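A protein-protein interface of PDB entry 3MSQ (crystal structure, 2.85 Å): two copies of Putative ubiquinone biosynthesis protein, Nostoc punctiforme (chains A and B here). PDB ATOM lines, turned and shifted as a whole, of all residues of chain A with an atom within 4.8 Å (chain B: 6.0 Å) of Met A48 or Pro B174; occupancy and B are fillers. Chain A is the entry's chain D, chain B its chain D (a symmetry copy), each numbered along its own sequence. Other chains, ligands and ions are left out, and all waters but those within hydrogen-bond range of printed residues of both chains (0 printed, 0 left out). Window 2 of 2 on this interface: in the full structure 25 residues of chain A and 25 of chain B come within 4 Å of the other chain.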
ATOM      1  N   THR A  46      -1.780  11.630 -28.549  1.00  0.00           N
ATOM      2  CA  THR A  46      -1.776  10.843 -27.312  1.00  0.00           C
ATOM      3  C   THR A  46      -2.697   9.609 -27.387  1.00  0.00           C
ATOM      4  O   THR A  46      -3.557   9.514 -28.266  1.00  0.00           O
ATOM      5  CB  THR A  46      -2.140  11.726 -26.095  1.00  0.00           C
ATOM      6  OG1 THR A  46      -3.517  12.072 -26.186  1.00  0.00           O
ATOM      7  CG2 THR A  46      -1.271  12.998 -25.983  1.00  0.00           C
ATOM      8  N   GLN A  47      -2.518   8.684 -26.430  1.00  0.00           N
ATOM      9  CA  GLN A  47      -3.313   7.469 -26.295  1.00  0.00           C
ATOM     10  C   GLN A  47      -4.735   7.781 -25.803  1.00  0.00           C
ATOM     11  O   GLN A  47      -5.683   7.105 -26.213  1.00  0.00           O
ATOM     12  CB  GLN A  47      -2.621   6.500 -25.335  1.00  0.00           C
ATOM     13  CG  GLN A  47      -3.217   5.109 -25.367  1.00  0.00           C
ATOM     14  CD  GLN A  47      -2.707   4.224 -24.270  1.00  0.00           C
ATOM     15  OE1 GLN A  47      -1.574   4.353 -23.789  1.00  0.00           O
ATOM     16  NE2 GLN A  47      -3.541   3.283 -23.857  1.00  0.00           N
ATOM     17  N   MET A  48      -4.875   8.789 -24.910  1.00  0.00           N
ATOM     18  CA  MET A  48      -6.150   9.227 -24.348  1.00  0.00           C
ATOM     19  C   MET A  48      -7.086   9.723 -25.456  1.00  0.00           C
ATOM     20  O   MET A  48      -8.291   9.531 -25.334  1.00  0.00           O
ATOM     21  CB  MET A  48      -5.913  10.294 -23.256  1.00  0.00           C
ATOM     22  CG  MET A  48      -7.200  10.971 -22.726  1.00  0.00           C
ATOM     23  SD  MET A  48      -7.839  10.493 -20.925  1.00  0.00           S
ATOM     24  CE  MET A  48      -9.605  11.345 -20.971  1.00  0.00           C
ATOM     25  N   ALA A  49      -6.539  10.320 -26.541  1.00  0.00           N
ATOM     26  CA  ALA A  49      -7.309  10.815 -27.688  1.00  0.00           C
ATOM     27  C   ALA A  49      -8.056   9.648 -28.320  1.00  0.00           C
ATOM     28  O   ALA A  49      -9.274   9.717 -28.461  1.00  0.00           O
ATOM     29  CB  ALA A  49      -6.392  11.487 -28.711  1.00  0.00           C
ATOM     30  N   GLN A  50      -7.343   8.553 -28.617  1.00  0.00           N
ATOM     31  CA  GLN A  50      -7.904   7.345 -29.217  1.00  0.00           C
ATOM     32  C   GLN A  50      -8.879   6.623 -28.291  1.00  0.00           C
ATOM     33  O   GLN A  50      -9.934   6.169 -28.743  1.00  0.00           O
ATOM     34  CB  GLN A  50      -6.786   6.399 -29.680  1.00  0.00           C
ATOM     35  CG  GLN A  50      -7.265   5.295 -30.630  1.00  0.00           C
ATOM     36  CD  GLN A  50      -8.064   5.821 -31.801  1.00  0.00           C
ATOM     37  OE1 GLN A  50      -7.584   6.605 -32.628  1.00  0.00           O
ATOM     38  NE2 GLN A  50      -9.320   5.425 -31.871  1.00  0.00           N
ATOM     39  N   LEU A  51      -8.517   6.513 -27.007  1.00  0.00           N
ATOM     40  CA  LEU A  51      -9.324   5.873 -25.975  1.00  0.00           C
ATOM     41  C   LEU A  51     -10.666   6.575 -25.799  1.00  0.00           C
ATOM     42  O   LEU A  51     -11.691   5.895 -25.708  1.00  0.00           O
ATOM     43  CB  LEU A  51      -8.554   5.890 -24.667  1.00  0.00           C
ATOM     44  CG  LEU A  51      -8.525   4.591 -23.912  1.00  0.00           C
ATOM     45  CD1 LEU A  51      -7.285   3.740 -24.315  1.00  0.00           C
ATOM     46  CD2 LEU A  51      -8.596   4.863 -22.408  1.00  0.00           C
ATOM     47  N   ALA A  52     -10.661   7.932 -25.793  1.00  0.00           N
ATOM     48  CA  ALA A  52     -11.861   8.773 -25.693  1.00  0.00           C
ATOM     49  C   ALA A  52     -12.824   8.460 -26.852  1.00  0.00           C
ATOM     50  O   ALA A  52     -14.016   8.260 -26.624  1.00  0.00           O
ATOM     51  CB  ALA A  52     -11.477  10.251 -25.703  1.00  0.00           C
ATOM     52  N   PRO A 154     -15.587  11.556 -20.536  1.00  0.00           N
ATOM     53  CA  PRO A 154     -14.205  12.090 -20.484  1.00  0.00           C
ATOM     54  C   PRO A 154     -13.430  12.116 -21.802  1.00  0.00           C
ATOM     55  O   PRO A 154     -13.305  11.102 -22.483  1.00  0.00           O
ATOM     56  CB  PRO A 154     -13.493  11.216 -19.441  1.00  0.00           C
ATOM     57  CG  PRO A 154     -14.492  10.285 -18.918  1.00  0.00           C
ATOM     58  CD  PRO A 154     -15.737  10.329 -19.725  1.00  0.00           C
ATOM     59  N   ILE A 155     -12.911  13.306 -22.147  1.00  0.00           N
ATOM     60  CA  ILE A 155     -12.065  13.555 -23.323  1.00  0.00           C
ATOM     61  C   ILE A 155     -10.797  14.291 -22.848  1.00  0.00           C
ATOM     62  O   ILE A 155     -10.878  15.012 -21.857  1.00  0.00           O
ATOM     63  CB  ILE A 155     -12.791  14.257 -24.523  1.00  0.00           C
ATOM     64  CG1 ILE A 155     -13.176  15.714 -24.205  1.00  0.00           C
ATOM     65  CG2 ILE A 155     -13.978  13.421 -25.051  1.00  0.00           C
ATOM     66  CD1 ILE A 155     -13.508  16.584 -25.406  1.00  0.00           C
ATOM     67  N   PRO A 156      -9.614  14.090 -23.488  1.00  0.00           N
ATOM     68  CA  PRO A 156      -8.378  14.731 -22.988  1.00  0.00           C
ATOM     69  C   PRO A 156      -8.407  16.197 -22.549  1.00  0.00           C
ATOM     70  O   PRO A 156      -7.971  16.476 -21.431  1.00  0.00           O
ATOM     71  CB  PRO A 156      -7.346  14.446 -24.091  1.00  0.00           C
ATOM     72  CG  PRO A 156      -8.093  13.794 -25.215  1.00  0.00           C
ATOM     73  CD  PRO A 156      -9.320  13.204 -24.637  1.00  0.00           C
ATOM     74  N   VAL A 159      -9.812  17.011 -18.987  1.00  0.00           N
ATOM     75  CA  VAL A 159      -8.883  16.604 -17.914  1.00  0.00           C
ATOM     76  C   VAL A 159      -7.806  17.668 -17.736  1.00  0.00           C
ATOM     77  O   VAL A 159      -7.508  18.071 -16.605  1.00  0.00           O
ATOM     78  CB  VAL A 159      -8.190  15.263 -18.244  1.00  0.00           C
ATOM     79  CG1 VAL A 159      -7.456  14.708 -17.027  1.00  0.00           C
ATOM     80  CG2 VAL A 159      -9.172  14.256 -18.814  1.00  0.00           C
ATOM     81  N   ILE B 169      -1.800  10.189 -15.199  1.00  0.00           N
ATOM     82  CA  ILE B 169      -2.585   8.999 -15.518  1.00  0.00           C
ATOM     83  C   ILE B 169      -3.188   9.132 -16.915  1.00  0.00           C
ATOM     84  O   ILE B 169      -2.985   8.246 -17.732  1.00  0.00           O
ATOM     85  CB  ILE B 169      -3.628   8.632 -14.423  1.00  0.00           C
ATOM     86  CG1 ILE B 169      -2.985   8.450 -13.001  1.00  0.00           C
ATOM     87  CG2 ILE B 169      -4.543   7.444 -14.843  1.00  0.00           C
ATOM     88  CD1 ILE B 169      -1.857   7.486 -12.877  1.00  0.00           C
ATOM     89  N   SER B 170      -3.871  10.250 -17.217  1.00  0.00           N
ATOM     90  CA  SER B 170      -4.443  10.444 -18.557  1.00  0.00           C
ATOM     91  C   SER B 170      -3.384  10.457 -19.677  1.00  0.00           C
ATOM     92  O   SER B 170      -3.627   9.891 -20.745  1.00  0.00           O
ATOM     93  CB  SER B 170      -5.357  11.665 -18.608  1.00  0.00           C
ATOM     94  OG  SER B 170      -4.705  12.786 -18.049  1.00  0.00           O
ATOM     95  N   LEU B 171      -2.193  11.014 -19.412  1.00  0.00           N
ATOM     96  CA  LEU B 171      -1.114  11.017 -20.415  1.00  0.00           C
ATOM     97  C   LEU B 171      -0.440   9.657 -20.585  1.00  0.00           C
ATOM     98  O   LEU B 171      -0.381   9.161 -21.698  1.00  0.00           O
ATOM     99  CB  LEU B 171      -0.041  12.097 -20.141  1.00  0.00           C
ATOM    100  CG  LEU B 171      -0.411  13.515 -20.493  1.00  0.00           C
ATOM    101  CD1 LEU B 171       0.600  14.467 -19.957  1.00  0.00           C
ATOM    102  CD2 LEU B 171      -0.540  13.704 -21.994  1.00  0.00           C
ATOM    103  N   TYR B 172       0.036   9.053 -19.480  1.00  0.00           N
ATOM    104  CA  TYR B 172       0.804   7.819 -19.496  1.00  0.00           C
ATOM    105  C   TYR B 172       0.101   6.478 -19.288  1.00  0.00           C
ATOM    106  O   TYR B 172       0.602   5.466 -19.774  1.00  0.00           O
ATOM    107  CB  TYR B 172       2.061   7.974 -18.644  1.00  0.00           C
ATOM    108  CG  TYR B 172       2.937   9.113 -19.122  1.00  0.00           C
ATOM    109  CD1 TYR B 172       3.794   8.951 -20.208  1.00  0.00           C
ATOM    110  CD2 TYR B 172       2.881  10.360 -18.512  1.00  0.00           C
ATOM    111  CE1 TYR B 172       4.596   9.996 -20.656  1.00  0.00           C
ATOM    112  CE2 TYR B 172       3.672  11.418 -18.958  1.00  0.00           C
ATOM    113  CZ  TYR B 172       4.541  11.226 -20.025  1.00  0.00           C
ATOM    114  OH  TYR B 172       5.344  12.249 -20.469  1.00  0.00           O
ATOM    115  N   GLN B 173      -1.022   6.448 -18.577  1.00  0.00           N
ATOM    116  CA  GLN B 173      -1.786   5.216 -18.379  1.00  0.00           C
ATOM    117  C   GLN B 173      -3.296   5.505 -18.465  1.00  0.00           C
ATOM    118  O   GLN B 173      -4.019   5.322 -17.485  1.00  0.00           O
ATOM    119  CB  GLN B 173      -1.369   4.454 -17.102  1.00  0.00           C
ATOM    120  CG  GLN B 173      -1.210   5.290 -15.838  1.00  0.00           C
ATOM    121  CD  GLN B 173      -0.783   4.427 -14.685  1.00  0.00           C
ATOM    122  OE1 GLN B 173      -1.525   3.539 -14.222  1.00  0.00           O
ATOM    123  NE2 GLN B 173       0.425   4.674 -14.194  1.00  0.00           N
ATOM    124  N   PRO B 174      -3.783   6.007 -19.635  1.00  0.00           N
ATOM    125  CA  PRO B 174      -5.196   6.392 -19.738  1.00  0.00           C
ATOM    126  C   PRO B 174      -6.212   5.280 -19.540  1.00  0.00           C
ATOM    127  O   PRO B 174      -7.355   5.587 -19.186  1.00  0.00           O
ATOM    128  CB  PRO B 174      -5.281   7.044 -21.119  1.00  0.00           C
ATOM    129  CG  PRO B 174      -4.173   6.437 -21.884  1.00  0.00           C
ATOM    130  CD  PRO B 174      -3.071   6.297 -20.900  1.00  0.00           C
ATOM    131  N   THR B 175      -5.802   4.000 -19.701  1.00  0.00           N
ATOM    132  CA  THR B 175      -6.685   2.840 -19.486  1.00  0.00           C
ATOM    133  C   THR B 175      -7.124   2.713 -18.014  1.00  0.00           C
ATOM    134  O   THR B 175      -8.042   1.960 -17.706  1.00  0.00           O
ATOM    135  CB  THR B 175      -6.047   1.543 -20.018  1.00  0.00           C
ATOM    136  OG1 THR B 175      -4.737   1.390 -19.466  1.00  0.00           O
ATOM    137  CG2 THR B 175      -5.982   1.513 -21.529  1.00  0.00           C
ATOM    138  N   ASN B 176      -6.479   3.479 -17.119  1.00  0.00           N
ATOM    139  CA  ASN B 176      -6.739   3.500 -15.685  1.00  0.00           C
ATOM    140  C   ASN B 176      -7.318   4.832 -15.201  1.00  0.00           C
ATOM    141  O   ASN B 176      -7.387   5.052 -13.985  1.00  0.00           O
ATOM    142  CB  ASN B 176      -5.458   3.175 -14.927  1.00  0.00           C
ATOM    143  CG  ASN B 176      -4.929   1.788 -15.143  1.00  0.00           C
ATOM    144  OD1 ASN B 176      -5.674   0.794 -15.241  1.00  0.00           O
ATOM    145  ND2 ASN B 176      -3.611   1.701 -15.218  1.00  0.00           N
ATOM    146  N   PHE B 177      -7.750   5.707 -16.141  1.00  0.00           N
ATOM    147  CA  PHE B 177      -8.323   7.013 -15.817  1.00  0.00           C
ATOM    148  C   PHE B 177      -9.667   6.903 -15.063  1.00  0.00           C
ATOM    149  O   PHE B 177      -9.841   7.578 -14.044  1.00  0.00           O
ATOM    150  CB  PHE B 177      -8.402   7.927 -17.056  1.00  0.00           C
ATOM    151  CG  PHE B 177      -8.797   9.351 -16.731  1.00  0.00           C
ATOM    152  CD1 PHE B 177      -7.897  10.219 -16.110  1.00  0.00           C
ATOM    153  CD2 PHE B 177     -10.079   9.818 -17.017  1.00  0.00           C
ATOM    154  CE1 PHE B 177      -8.271  11.531 -15.787  1.00  0.00           C
ATOM    155  CE2 PHE B 177     -10.454  11.130 -16.695  1.00  0.00           C
ATOM    156  CZ  PHE B 177      -9.549  11.973 -16.075  1.00  0.00           C
ATOM    157  N   LYS B 178     -10.580   6.021 -15.527  1.00  0.00           N
ATOM    158  CA  LYS B 178     -11.887   5.791 -14.888  1.00  0.00           C
ATOM    159  C   LYS B 178     -11.692   5.391 -13.408  1.00  0.00           C
ATOM    160  O   LYS B 178     -12.386   5.902 -12.524  1.00  0.00           O
ATOM    161  CB  LYS B 178     -12.692   4.720 -15.654  1.00  0.00           C
ATOM    162  CG  LYS B 178     -14.153   4.589 -15.208  1.00  0.00           C
ATOM    163  CD  LYS B 178     -14.859   3.330 -15.747  1.00  0.00           C
ATOM    164  CE  LYS B 178     -16.287   3.263 -15.258  1.00  0.00           C
ATOM    165  NZ  LYS B 178     -16.887   1.917 -15.444  1.00  0.00           N
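Gln A47 touches Pro B174 (CD to CG, 3.6 Å). NE2 of Gln A47 touches CG2 of Thr B175, at 3.8 Å. Ser B170 touches Met A48 (O to CB, 3.4 Å). Met A48 touches Pro B174. Leu A51 touches Pro B174. CG2 of Thr B175 touches CD1 of Leu A51, 3.8 Å away. Val A159 touches Ser B170 (CG1 to OG, 3.5 Å). Val A159 touches Phe B177 (CG1 to CE1, 3.5 Å).
Met A48 touches two residues of chain B. Pro B174 touches just these residues of chain A: Gln A47 (3.6 Å), Met A48 (3.9 Å) and Leu A51 (3.5 Å). Of the printed residues of chain A, Ser B170 touches Met A48 (3.4 Å) and Val A159 (3.5 Å). Of the printed residues of chain B, Leu A51 touches Pro B174 (3.5 Å) and Thr B175 (3.8 Å). Gln B173 touches none of the printed residues of chain A. Thr A46 touches none of the printed residues of chain B.
Printed residues of chain A that touch a printed residue of chain B: Gln A47, Met A48, Leu A51 and Val A159. Hydrophobic or aromatic side chains of chain A that line the printed part of chain B: Met A48, Leu A51 and Val A159. Of the 10 printed residues of chain B, 4 touch a printed residue of chain A. Among the printed residues, 8 pairs touch across the chains. Among the printed residues, no Asp or Glu carboxylate lies within 4 Å of a Lys or Arg side-chain nitrogen of the other chain.
No position is printed for both chains.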
